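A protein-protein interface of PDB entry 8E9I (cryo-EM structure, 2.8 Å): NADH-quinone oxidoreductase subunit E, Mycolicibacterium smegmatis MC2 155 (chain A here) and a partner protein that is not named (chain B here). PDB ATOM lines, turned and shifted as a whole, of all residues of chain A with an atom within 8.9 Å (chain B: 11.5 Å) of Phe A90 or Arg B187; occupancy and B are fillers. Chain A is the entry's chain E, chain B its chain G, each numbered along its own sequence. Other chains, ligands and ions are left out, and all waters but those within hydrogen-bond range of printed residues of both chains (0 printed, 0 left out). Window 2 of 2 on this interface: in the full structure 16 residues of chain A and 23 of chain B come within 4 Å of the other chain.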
ATOM      1  N   ILE A  19     -25.634 -17.928   1.194  1.00  0.00           N
ATOM      2  CA  ILE A  19     -25.454 -17.003   2.301  1.00  0.00           C
ATOM      3  C   ILE A  19     -26.783 -16.320   2.577  1.00  0.00           C
ATOM      4  O   ILE A  19     -27.315 -15.599   1.724  1.00  0.00           O
ATOM      5  CB  ILE A  19     -24.356 -15.986   1.983  1.00  0.00           C
ATOM      6  CG1 ILE A  19     -23.014 -16.688   1.769  1.00  0.00           C
ATOM      7  CG2 ILE A  19     -24.253 -14.965   3.090  1.00  0.00           C
ATOM      8  CD1 ILE A  19     -22.391 -17.224   3.030  1.00  0.00           C
ATOM      9  N   LEU A  52      -9.807 -13.142   3.936  1.00  0.00           N
ATOM     10  CA  LEU A  52     -10.031 -14.443   4.566  1.00  0.00           C
ATOM     11  C   LEU A  52     -10.076 -14.333   6.082  1.00  0.00           C
ATOM     12  O   LEU A  52     -11.014 -14.867   6.698  1.00  0.00           O
ATOM     13  CB  LEU A  52      -8.958 -15.427   4.102  1.00  0.00           C
ATOM     14  CG  LEU A  52      -9.377 -16.395   2.995  1.00  0.00           C
ATOM     15  CD1 LEU A  52      -9.791 -15.637   1.755  1.00  0.00           C
ATOM     16  CD2 LEU A  52      -8.246 -17.350   2.676  1.00  0.00           C
ATOM     17  N   LEU A  55     -13.361 -12.487   7.005  1.00  0.00           N
ATOM     18  CA  LEU A  55     -14.534 -13.349   6.933  1.00  0.00           C
ATOM     19  C   LEU A  55     -14.651 -14.212   8.182  1.00  0.00           C
ATOM     20  O   LEU A  55     -15.720 -14.276   8.799  1.00  0.00           O
ATOM     21  CB  LEU A  55     -14.478 -14.219   5.682  1.00  0.00           C
ATOM     22  CG  LEU A  55     -14.873 -13.491   4.401  1.00  0.00           C
ATOM     23  CD1 LEU A  55     -14.417 -14.274   3.194  1.00  0.00           C
ATOM     24  CD2 LEU A  55     -16.370 -13.268   4.356  1.00  0.00           C
ATOM     25  N   LEU A  65     -21.482 -17.638   8.188  1.00  0.00           N
ATOM     26  CA  LEU A  65     -21.506 -16.458   7.339  1.00  0.00           C
ATOM     27  C   LEU A  65     -22.938 -16.066   7.008  1.00  0.00           C
ATOM     28  O   LEU A  65     -23.778 -16.913   6.698  1.00  0.00           O
ATOM     29  CB  LEU A  65     -20.727 -16.699   6.050  1.00  0.00           C
ATOM     30  CG  LEU A  65     -19.200 -16.661   6.136  1.00  0.00           C
ATOM     31  CD1 LEU A  65     -18.630 -16.456   4.758  1.00  0.00           C
ATOM     32  CD2 LEU A  65     -18.697 -15.576   7.069  1.00  0.00           C
ATOM     33  N   GLU A  83     -18.185  -9.924  -5.011  1.00  0.00           N
ATOM     34  CA  GLU A  83     -16.821 -10.440  -4.917  1.00  0.00           C
ATOM     35  C   GLU A  83     -16.579 -11.100  -3.569  1.00  0.00           C
ATOM     36  O   GLU A  83     -15.943 -12.162  -3.485  1.00  0.00           O
ATOM     37  CB  GLU A  83     -15.818  -9.312  -5.146  1.00  0.00           C
ATOM     38  N   VAL A  84     -17.074 -10.483  -2.500  1.00  0.00           N
ATOM     39  CA  VAL A  84     -16.914 -11.059  -1.173  1.00  0.00           C
ATOM     40  C   VAL A  84     -17.621 -12.403  -1.100  1.00  0.00           C
ATOM     41  O   VAL A  84     -17.091 -13.372  -0.552  1.00  0.00           O
ATOM     42  CB  VAL A  84     -17.436 -10.088  -0.100  1.00  0.00           C
ATOM     43  CG1 VAL A  84     -17.308 -10.709   1.274  1.00  0.00           C
ATOM     44  CG2 VAL A  84     -16.688  -8.772  -0.168  1.00  0.00           C
ATOM     45  N   THR A  85     -18.833 -12.479  -1.647  1.00  0.00           N
ATOM     46  CA  THR A  85     -19.550 -13.747  -1.662  1.00  0.00           C
ATOM     47  C   THR A  85     -18.785 -14.795  -2.451  1.00  0.00           C
ATOM     48  O   THR A  85     -18.684 -15.952  -2.031  1.00  0.00           O
ATOM     49  CB  THR A  85     -20.939 -13.555  -2.258  1.00  0.00           C
ATOM     50  OG1 THR A  85     -21.642 -12.550  -1.521  1.00  0.00           O
ATOM     51  CG2 THR A  85     -21.720 -14.851  -2.218  1.00  0.00           C
ATOM     52  N   ALA A  86     -18.246 -14.409  -3.603  1.00  0.00           N
ATOM     53  CA  ALA A  86     -17.472 -15.345  -4.400  1.00  0.00           C
ATOM     54  C   ALA A  86     -16.328 -15.922  -3.592  1.00  0.00           C
ATOM     55  O   ALA A  86     -16.140 -17.143  -3.556  1.00  0.00           O
ATOM     56  CB  ALA A  86     -16.947 -14.651  -5.655  1.00  0.00           C
ATOM     57  N   VAL A  87     -15.561 -15.067  -2.922  1.00  0.00           N
ATOM     58  CA  VAL A  87     -14.467 -15.575  -2.101  1.00  0.00           C
ATOM     59  C   VAL A  87     -15.008 -16.472  -0.996  1.00  0.00           C
ATOM     60  O   VAL A  87     -14.496 -17.570  -0.756  1.00  0.00           O
ATOM     61  CB  VAL A  87     -13.639 -14.416  -1.528  1.00  0.00           C
ATOM     62  CG1 VAL A  87     -12.628 -14.940  -0.535  1.00  0.00           C
ATOM     63  CG2 VAL A  87     -12.942 -13.673  -2.642  1.00  0.00           C
ATOM     64  N   ALA A  88     -16.065 -16.027  -0.319  1.00  0.00           N
ATOM     65  CA  ALA A  88     -16.579 -16.771   0.824  1.00  0.00           C
ATOM     66  C   ALA A  88     -17.098 -18.139   0.413  1.00  0.00           C
ATOM     67  O   ALA A  88     -16.744 -19.152   1.022  1.00  0.00           O
ATOM     68  CB  ALA A  88     -17.683 -15.973   1.512  1.00  0.00           C
ATOM     69  N   THR A  89     -17.937 -18.196  -0.615  1.00  0.00           N
ATOM     70  CA  THR A  89     -18.513 -19.471  -1.008  1.00  0.00           C
ATOM     71  C   THR A  89     -17.463 -20.459  -1.485  1.00  0.00           C
ATOM     72  O   THR A  89     -17.751 -21.656  -1.558  1.00  0.00           O
ATOM     73  CB  THR A  89     -19.549 -19.266  -2.109  1.00  0.00           C
ATOM     74  OG1 THR A  89     -18.950 -18.556  -3.198  1.00  0.00           O
ATOM     75  CG2 THR A  89     -20.731 -18.478  -1.585  1.00  0.00           C
ATOM     76  N   PHE A  90     -16.260 -19.990  -1.807  1.00  0.00           N
ATOM     77  CA  PHE A  90     -15.231 -20.881  -2.326  1.00  0.00           C
ATOM     78  C   PHE A  90     -14.707 -21.810  -1.237  1.00  0.00           C
ATOM     79  O   PHE A  90     -14.523 -23.009  -1.466  1.00  0.00           O
ATOM     80  CB  PHE A  90     -14.101 -20.051  -2.930  1.00  0.00           C
ATOM     81  CG  PHE A  90     -13.078 -20.856  -3.663  1.00  0.00           C
ATOM     82  CD1 PHE A  90     -13.302 -21.253  -4.967  1.00  0.00           C
ATOM     83  CD2 PHE A  90     -11.881 -21.189  -3.066  1.00  0.00           C
ATOM     84  CE1 PHE A  90     -12.361 -21.984  -5.650  1.00  0.00           C
ATOM     85  CE2 PHE A  90     -10.940 -21.918  -3.746  1.00  0.00           C
ATOM     86  CZ  PHE A  90     -11.179 -22.314  -5.041  1.00  0.00           C
ATOM     87  N   TYR A  91     -14.475 -21.279  -0.044  1.00  0.00           N
ATOM     88  CA  TYR A  91     -13.859 -22.063   1.014  1.00  0.00           C
ATOM     89  C   TYR A  91     -14.905 -22.755   1.877  1.00  0.00           C
ATOM     90  O   TYR A  91     -15.970 -22.208   2.171  1.00  0.00           O
ATOM     91  CB  TYR A  91     -12.968 -21.177   1.875  1.00  0.00           C
ATOM     92  CG  TYR A  91     -11.952 -20.429   1.064  1.00  0.00           C
ATOM     93  CD1 TYR A  91     -12.259 -19.213   0.482  1.00  0.00           C
ATOM     94  CD2 TYR A  91     -10.689 -20.949   0.862  1.00  0.00           C
ATOM     95  CE1 TYR A  91     -11.328 -18.533  -0.267  1.00  0.00           C
ATOM     96  CE2 TYR A  91      -9.763 -20.278   0.118  1.00  0.00           C
ATOM     97  CZ  TYR A  91     -10.082 -19.077  -0.446  1.00  0.00           C
ATOM     98  OH  TYR A  91      -9.138 -18.418  -1.191  1.00  0.00           O
ATOM     99  N   SER A  92     -14.581 -23.983   2.280  1.00  0.00           N
ATOM    100  CA  SER A  92     -15.515 -24.801   3.038  1.00  0.00           C
ATOM    101  C   SER A  92     -15.607 -24.379   4.495  1.00  0.00           C
ATOM    102  O   SER A  92     -16.658 -24.558   5.118  1.00  0.00           O
ATOM    103  CB  SER A  92     -15.099 -26.266   2.950  1.00  0.00           C
ATOM    104  OG  SER A  92     -13.794 -26.442   3.466  1.00  0.00           O
ATOM    105  N   MET A  93     -14.533 -23.829   5.056  1.00  0.00           N
ATOM    106  CA  MET A  93     -14.539 -23.492   6.475  1.00  0.00           C
ATOM    107  C   MET A  93     -15.550 -22.405   6.793  1.00  0.00           C
ATOM    108  O   MET A  93     -15.931 -22.236   7.955  1.00  0.00           O
ATOM    109  CB  MET A  93     -13.142 -23.064   6.898  1.00  0.00           C
ATOM    110  CG  MET A  93     -12.198 -24.221   6.896  1.00  0.00           C
ATOM    111  SD  MET A  93     -10.726 -24.032   7.886  1.00  0.00           S
ATOM    112  CE  MET A  93      -9.664 -25.070   6.890  1.00  0.00           C
ATOM    113  N   TYR A  94     -15.986 -21.657   5.787  1.00  0.00           N
ATOM    114  CA  TYR A  94     -17.013 -20.638   5.973  1.00  0.00           C
ATOM    115  C   TYR A  94     -18.372 -21.325   5.915  1.00  0.00           C
ATOM    116  O   TYR A  94     -19.007 -21.447   4.866  1.00  0.00           O
ATOM    117  CB  TYR A  94     -16.866 -19.547   4.924  1.00  0.00           C
ATOM    118  CG  TYR A  94     -15.540 -18.837   5.017  1.00  0.00           C
ATOM    119  CD1 TYR A  94     -15.102 -18.315   6.222  1.00  0.00           C
ATOM    120  CD2 TYR A  94     -14.719 -18.705   3.912  1.00  0.00           C
ATOM    121  CE1 TYR A  94     -13.894 -17.672   6.320  1.00  0.00           C
ATOM    122  CE2 TYR A  94     -13.505 -18.065   4.003  1.00  0.00           C
ATOM    123  CZ  TYR A  94     -13.099 -17.552   5.208  1.00  0.00           C
ATOM    124  OH  TYR A  94     -11.890 -16.909   5.310  1.00  0.00           O
ATOM    125  N   ARG A  96     -22.275 -22.068   6.224  1.00  0.00           N
ATOM    126  CA  ARG A  96     -23.384 -21.265   5.731  1.00  0.00           C
ATOM    127  C   ARG A  96     -24.699 -21.610   6.414  1.00  0.00           C
ATOM    128  O   ARG A  96     -25.764 -21.428   5.815  1.00  0.00           O
ATOM    129  CB  ARG A  96     -23.500 -21.431   4.217  1.00  0.00           C
ATOM    130  CG  ARG A  96     -22.145 -21.367   3.540  1.00  0.00           C
ATOM    131  CD  ARG A  96     -22.215 -20.801   2.146  1.00  0.00           C
ATOM    132  NE  ARG A  96     -23.021 -21.623   1.258  1.00  0.00           N
ATOM    133  CZ  ARG A  96     -22.585 -22.185   0.139  1.00  0.00           C
ATOM    134  NH1 ARG A  96     -21.319 -22.097  -0.235  1.00  0.00           N
ATOM    135  NH2 ARG A  96     -23.440 -22.858  -0.622  1.00  0.00           N
ATOM    136  N   GLU A 147     -12.581 -33.594   4.558  1.00  0.00           N
ATOM    137  CA  GLU A 147     -11.588 -34.259   3.726  1.00  0.00           C
ATOM    138  C   GLU A 147     -10.320 -34.467   4.539  1.00  0.00           C
ATOM    139  O   GLU A 147     -10.311 -34.217   5.747  1.00  0.00           O
ATOM    140  CB  GLU A 147     -11.297 -33.447   2.465  1.00  0.00           C
ATOM    141  N   ASN B 109     -23.107 -32.172 -18.452  1.00  0.00           N
ATOM    142  CA  ASN B 109     -24.008 -31.537 -17.504  1.00  0.00           C
ATOM    143  C   ASN B 109     -24.922 -30.508 -18.151  1.00  0.00           C
ATOM    144  O   ASN B 109     -25.751 -29.915 -17.457  1.00  0.00           O
ATOM    145  CB  ASN B 109     -23.203 -30.864 -16.396  1.00  0.00           C
ATOM    146  CG  ASN B 109     -22.796 -31.826 -15.308  1.00  0.00           C
ATOM    147  OD1 ASN B 109     -23.528 -32.753 -14.972  1.00  0.00           O
ATOM    148  ND2 ASN B 109     -21.621 -31.607 -14.742  1.00  0.00           N
ATOM    149  N   ARG B 144     -25.832 -32.488 -13.664  1.00  0.00           N
ATOM    150  CA  ARG B 144     -25.944 -31.453 -12.650  1.00  0.00           C
ATOM    151  C   ARG B 144     -27.182 -30.620 -12.925  1.00  0.00           C
ATOM    152  O   ARG B 144     -27.566 -30.418 -14.079  1.00  0.00           O
ATOM    153  CB  ARG B 144     -24.709 -30.557 -12.652  1.00  0.00           C
ATOM    154  CG  ARG B 144     -24.815 -29.380 -11.701  1.00  0.00           C
ATOM    155  CD  ARG B 144     -23.552 -28.557 -11.698  1.00  0.00           C
ATOM    156  NE  ARG B 144     -23.356 -27.885 -12.977  1.00  0.00           N
ATOM    157  CZ  ARG B 144     -22.248 -27.929 -13.703  1.00  0.00           C
ATOM    158  NH1 ARG B 144     -21.187 -28.620 -13.315  1.00  0.00           N
ATOM    159  NH2 ARG B 144     -22.199 -27.256 -14.848  1.00  0.00           N
ATOM    160  N   THR B 145     -27.812 -30.129 -11.867  1.00  0.00           N
ATOM    161  CA  THR B 145     -29.058 -29.399 -12.018  1.00  0.00           C
ATOM    162  C   THR B 145     -29.082 -28.206 -11.076  1.00  0.00           C
ATOM    163  O   THR B 145     -28.667 -28.307  -9.919  1.00  0.00           O
ATOM    164  CB  THR B 145     -30.263 -30.308 -11.748  1.00  0.00           C
ATOM    165  OG1 THR B 145     -31.475 -29.557 -11.876  1.00  0.00           O
ATOM    166  CG2 THR B 145     -30.187 -30.899 -10.347  1.00  0.00           C
ATOM    167  N   PHE B 146     -29.567 -27.081 -11.585  1.00  0.00           N
ATOM    168  CA  PHE B 146     -29.831 -25.886 -10.808  1.00  0.00           C
ATOM    169  C   PHE B 146     -31.271 -25.460 -11.030  1.00  0.00           C
ATOM    170  O   PHE B 146     -31.834 -25.709 -12.100  1.00  0.00           O
ATOM    171  CB  PHE B 146     -28.917 -24.722 -11.211  1.00  0.00           C
ATOM    172  CG  PHE B 146     -27.480 -24.917 -10.860  1.00  0.00           C
ATOM    173  CD1 PHE B 146     -27.032 -24.673  -9.580  1.00  0.00           C
ATOM    174  CD2 PHE B 146     -26.568 -25.301 -11.820  1.00  0.00           C
ATOM    175  CE1 PHE B 146     -25.709 -24.835  -9.258  1.00  0.00           C
ATOM    176  CE2 PHE B 146     -25.241 -25.460 -11.507  1.00  0.00           C
ATOM    177  CZ  PHE B 146     -24.810 -25.227 -10.225  1.00  0.00           C
ATOM    178  N   ARG B 160     -28.109 -21.362 -14.874  1.00  0.00           N
ATOM    179  CA  ARG B 160     -26.812 -21.859 -14.443  1.00  0.00           C
ATOM    180  C   ARG B 160     -26.458 -23.202 -15.052  1.00  0.00           C
ATOM    181  O   ARG B 160     -25.273 -23.475 -15.259  1.00  0.00           O
ATOM    182  CB  ARG B 160     -26.788 -21.947 -12.926  1.00  0.00           C
ATOM    183  CG  ARG B 160     -26.779 -20.595 -12.281  1.00  0.00           C
ATOM    184  CD  ARG B 160     -27.073 -20.678 -10.821  1.00  0.00           C
ATOM    185  NE  ARG B 160     -28.488 -20.915 -10.582  1.00  0.00           N
ATOM    186  CZ  ARG B 160     -29.007 -21.146  -9.389  1.00  0.00           C
ATOM    187  NH1 ARG B 160     -28.251 -21.188  -8.307  1.00  0.00           N
ATOM    188  NH2 ARG B 160     -30.318 -21.324  -9.275  1.00  0.00           N
ATOM    189  N   LEU B 165     -19.428 -21.915 -17.464  1.00  0.00           N
ATOM    190  CA  LEU B 165     -18.485 -21.342 -16.505  1.00  0.00           C
ATOM    191  C   LEU B 165     -17.222 -20.851 -17.195  1.00  0.00           C
ATOM    192  O   LEU B 165     -16.110 -21.056 -16.713  1.00  0.00           O
ATOM    193  CB  LEU B 165     -18.143 -22.342 -15.405  1.00  0.00           C
ATOM    194  CG  LEU B 165     -19.284 -22.616 -14.434  1.00  0.00           C
ATOM    195  CD1 LEU B 165     -19.131 -23.981 -13.797  1.00  0.00           C
ATOM    196  CD2 LEU B 165     -19.335 -21.537 -13.376  1.00  0.00           C
ATOM    197  N   ASP B 183     -20.011 -12.690  -9.810  1.00  0.00           N
ATOM    198  CA  ASP B 183     -18.731 -13.368  -9.756  1.00  0.00           C
ATOM    199  C   ASP B 183     -18.997 -14.859  -9.810  1.00  0.00           C
ATOM    200  O   ASP B 183     -20.130 -15.315  -9.647  1.00  0.00           O
ATOM    201  CB  ASP B 183     -17.949 -12.984  -8.500  1.00  0.00           C
ATOM    202  N   LEU B 184     -17.939 -15.611 -10.066  1.00  0.00           N
ATOM    203  CA  LEU B 184     -18.005 -17.050  -9.925  1.00  0.00           C
ATOM    204  C   LEU B 184     -18.064 -17.391  -8.444  1.00  0.00           C
ATOM    205  O   LEU B 184     -17.270 -16.889  -7.647  1.00  0.00           O
ATOM    206  CB  LEU B 184     -16.790 -17.698 -10.579  1.00  0.00           C
ATOM    207  CG  LEU B 184     -16.664 -17.453 -12.082  1.00  0.00           C
ATOM    208  CD1 LEU B 184     -15.472 -18.216 -12.626  1.00  0.00           C
ATOM    209  CD2 LEU B 184     -17.939 -17.829 -12.824  1.00  0.00           C
ATOM    210  N   MET B 185     -19.012 -18.247  -8.075  1.00  0.00           N
ATOM    211  CA  MET B 185     -19.325 -18.513  -6.683  1.00  0.00           C
ATOM    212  C   MET B 185     -19.422 -20.013  -6.481  1.00  0.00           C
ATOM    213  O   MET B 185     -19.494 -20.788  -7.437  1.00  0.00           O
ATOM    214  CB  MET B 185     -20.628 -17.821  -6.277  1.00  0.00           C
ATOM    215  CG  MET B 185     -20.520 -16.315  -6.274  1.00  0.00           C
ATOM    216  SD  MET B 185     -22.032 -15.472  -5.813  1.00  0.00           S
ATOM    217  CE  MET B 185     -21.489 -13.788  -6.032  1.00  0.00           C
ATOM    218  N   GLU B 186     -19.434 -20.420  -5.215  1.00  0.00           N
ATOM    219  CA  GLU B 186     -19.368 -21.831  -4.874  1.00  0.00           C
ATOM    220  C   GLU B 186     -18.054 -22.395  -5.388  1.00  0.00           C
ATOM    221  O   GLU B 186     -17.139 -21.635  -5.713  1.00  0.00           O
ATOM    222  CB  GLU B 186     -20.558 -22.592  -5.457  1.00  0.00           C
ATOM    223  N   ARG B 187     -17.947 -23.717  -5.477  1.00  0.00           N
ATOM    224  CA  ARG B 187     -16.681 -24.342  -5.820  1.00  0.00           C
ATOM    225  C   ARG B 187     -16.935 -25.669  -6.513  1.00  0.00           C
ATOM    226  O   ARG B 187     -18.016 -26.247  -6.402  1.00  0.00           O
ATOM    227  CB  ARG B 187     -15.829 -24.560  -4.571  1.00  0.00           C
ATOM    228  CG  ARG B 187     -14.467 -25.140  -4.836  1.00  0.00           C
ATOM    229  CD  ARG B 187     -13.536 -24.834  -3.697  1.00  0.00           C
ATOM    230  NE  ARG B 187     -13.959 -25.517  -2.481  1.00  0.00           N
ATOM    231  CZ  ARG B 187     -13.299 -26.503  -1.888  1.00  0.00           C
ATOM    232  NH1 ARG B 187     -12.141 -26.943  -2.351  1.00  0.00           N
ATOM    233  NH2 ARG B 187     -13.811 -27.058  -0.796  1.00  0.00           N
ATOM    234  N   GLY B 188     -15.921 -26.141  -7.229  1.00  0.00           N
ATOM    235  CA  GLY B 188     -16.003 -27.459  -7.827  1.00  0.00           C
ATOM    236  C   GLY B 188     -17.096 -27.519  -8.870  1.00  0.00           C
ATOM    237  O   GLY B 188     -17.400 -26.533  -9.547  1.00  0.00           O
ATOM    238  N   ALA B 189     -17.712 -28.692  -8.996  1.00  0.00           N
ATOM    239  CA  ALA B 189     -18.780 -28.853  -9.975  1.00  0.00           C
ATOM    240  C   ALA B 189     -19.926 -27.891  -9.710  1.00  0.00           C
ATOM    241  O   ALA B 189     -20.707 -27.591 -10.619  1.00  0.00           O
ATOM    242  CB  ALA B 189     -19.287 -30.292  -9.965  1.00  0.00           C
ATOM    243  N   LEU B 190     -20.037 -27.392  -8.485  1.00  0.00           N
ATOM    244  CA  LEU B 190     -21.131 -26.522  -8.091  1.00  0.00           C
ATOM    245  C   LEU B 190     -20.880 -25.058  -8.422  1.00  0.00           C
ATOM    246  O   LEU B 190     -21.731 -24.218  -8.120  1.00  0.00           O
ATOM    247  CB  LEU B 190     -21.385 -26.666  -6.590  1.00  0.00           C
ATOM    248  CG  LEU B 190     -22.688 -26.077  -6.062  1.00  0.00           C
ATOM    249  CD1 LEU B 190     -23.874 -26.712  -6.753  1.00  0.00           C
ATOM    250  CD2 LEU B 190     -22.778 -26.271  -4.566  1.00  0.00           C
ATOM    251  N   GLN B 191     -19.744 -24.728  -9.026  1.00  0.00           N
ATOM    252  CA  GLN B 191     -19.435 -23.333  -9.303  1.00  0.00           C
ATOM    253  C   GLN B 191     -20.498 -22.726 -10.207  1.00  0.00           C
ATOM    254  O   GLN B 191     -20.998 -23.375 -11.128  1.00  0.00           O
ATOM    255  CB  GLN B 191     -18.059 -23.211  -9.949  1.00  0.00           C
ATOM    256  CG  GLN B 191     -17.558 -21.793 -10.015  1.00  0.00           C
ATOM    257  CD  GLN B 191     -16.148 -21.697 -10.539  1.00  0.00           C
ATOM    258  OE1 GLN B 191     -15.218 -21.397  -9.793  1.00  0.00           O
ATOM    259  NE2 GLN B 191     -15.977 -21.948 -11.826  1.00  0.00           N
ATOM    260  N   GLN B 192     -20.849 -21.473  -9.937  1.00  0.00           N
ATOM    261  CA  GLN B 192     -21.944 -20.832 -10.647  1.00  0.00           C
ATOM    262  C   GLN B 192     -21.741 -19.328 -10.659  1.00  0.00           C
ATOM    263  O   GLN B 192     -21.313 -18.741  -9.668  1.00  0.00           O
ATOM    264  CB  GLN B 192     -23.286 -21.155  -9.992  1.00  0.00           C
ATOM    265  CG  GLN B 192     -23.371 -20.688  -8.557  1.00  0.00           C
ATOM    266  CD  GLN B 192     -24.533 -21.298  -7.821  1.00  0.00           C
ATOM    267  OE1 GLN B 192     -25.603 -20.706  -7.729  1.00  0.00           O
ATOM    268  NE2 GLN B 192     -24.333 -22.494  -7.294  1.00  0.00           N
ATOM    269  N   VAL B 193     -22.058 -18.702 -11.788  1.00  0.00           N
ATOM    270  CA  VAL B 193     -22.079 -17.250 -11.818  1.00  0.00           C
ATOM    271  C   VAL B 193     -23.234 -16.767 -10.956  1.00  0.00           C
ATOM    272  O   VAL B 193     -24.343 -17.309 -11.009  1.00  0.00           O
ATOM    273  CB  VAL B 193     -22.203 -16.723 -13.257  1.00  0.00           C
ATOM    274  CG1 VAL B 193     -23.533 -17.107 -13.846  1.00  0.00           C
ATOM    275  CG2 VAL B 193     -22.050 -15.227 -13.277  1.00  0.00           C
ATOM    276  N   GLY B 194     -22.979 -15.755 -10.137  1.00  0.00           N
ATOM    277  CA  GLY B 194     -24.024 -15.277  -9.256  1.00  0.00           C
ATOM    278  C   GLY B 194     -23.787 -13.861  -8.793  1.00  0.00           C
ATOM    279  O   GLY B 194     -22.659 -13.361  -8.795  1.00  0.00           O
ATOM    280  N   GLY B 196     -24.453 -11.151  -5.466  1.00  0.00           N
ATOM    281  CA  GLY B 196     -24.069 -11.406  -4.096  1.00  0.00           C
ATOM    282  C   GLY B 196     -25.114 -12.178  -3.321  1.00  0.00           C
ATOM    283  O   GLY B 196     -24.964 -13.387  -3.127  1.00  0.00           O
ATOM    284  N   GLN B 197     -26.184 -11.518  -2.886  1.00  0.00           N
ATOM    285  CA  GLN B 197     -27.305 -12.234  -2.295  1.00  0.00           C
ATOM    286  C   GLN B 197     -28.599 -11.872  -3.001  1.00  0.00           C
ATOM    287  O   GLN B 197     -29.296 -12.734  -3.545  1.00  0.00           O
ATOM    288  CB  GLN B 197     -27.396 -11.918  -0.803  1.00  0.00           C
ATOM    289  CG  GLN B 197     -26.392 -12.692   0.015  1.00  0.00           C
ATOM    290  CD  GLN B 197     -24.969 -12.253  -0.247  1.00  0.00           C
ATOM    291  OE1 GLN B 197     -24.669 -11.062  -0.277  1.00  0.00           O
ATOM    292  NE2 GLN B 197     -24.091 -13.219  -0.481  1.00  0.00           N
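The side-chain amide nitrogen (NE2) of Gln B197 lies within hydrogen-bond range of the side-chain hydroxyl (OG1) of Thr A85.
The side-chain hydroxyl (OG1) of Thr A89 sits at hydrogen-bond distance from the backbone NH (N) of Glu B186 (2.8 Å).
The guanidinium group (NE) of Arg B187 sits at hydrogen-bond distance from the backbone carbonyl oxygen (O) of Phe A90, at 2.8 Å.
The backbone carbonyl oxygen (O) of Ala A86 lies within hydrogen-bond range of the side-chain hydroxyl (OG1) of Thr A89 (3.2 Å).
The backbone carbonyl oxygen (O) of Thr A85 is in hydrogen-bond range of the side-chain hydroxyl (OG1) of Thr A89 (2.9 Å).
The backbone carbonyl oxygen of Gln B192 sits at hydrogen-bond distance from the backbone NH of Met B185, at 2.8 Å.
The backbone NH of Asp B183 is in hydrogen-bond range of the backbone carbonyl oxygen of Gly B194 (2.9 Å).
Among the printed residues, merely in contact across the chains: Ile A19 with Gln B197 (3.5 Å), Thr A85 with Met B185 (3.7 Å), Thr A85 with Gly B196 (3.7 Å), Ala A86 with Asp B183 (3.4 Å), Ala A86 with Leu B184 (3.0 Å), Ala A86 with Met B185 (3.7 Å), Thr A89 with Met B185 (3.5 Å) and Phe A90 with Glu B186 (3.9 Å).
Of the printed residues of chain B, Ile A19 touches Gln B197.
Ala A86 touches just these residues of chain B: Asp B183 (3.4 Å), Leu B184 (3.0 Å) and Met B185 (3.7 Å).
Val A87 touches none of the printed residues of chain B.
Of chain B, only Met B185 and Glu B186 come within 4 Å of Thr A89.
Printed residues of chain B within 4 Å of Phe A90: Glu B186 and Arg B187.
No residue of chain B comes within 4 Å of Tyr A91.
No residue of chain B comes within 4 Å of Ser A92.
Of the printed residues of chain A, Asp B183 touches Ala A86 (3.4 Å).
Printed residues of chain A within 4 Å of Met B185: Thr A85, Ala A86 and Thr A89.
No residue of chain A comes within 4 Å of Gly B188.
The nearest residue of chain A that does not touch Arg B187 is Ser A92 (4.04 Å).
The nearest printed residue of chain A that does not touch Met B185 is Glu A83 (5.2 Å).
Of the 20 printed residues of chain B, 7 touch a printed residue of chain A.
Hydrophobic or aromatic side chains of chain A that line the printed part of chain B: Ile A19, Ala A86 and Phe A90.
Along chain A the printed residues that touch a printed residue of chain B span positions 19 to 90.
Among the printed residues, 11 pairs touch across the chains.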
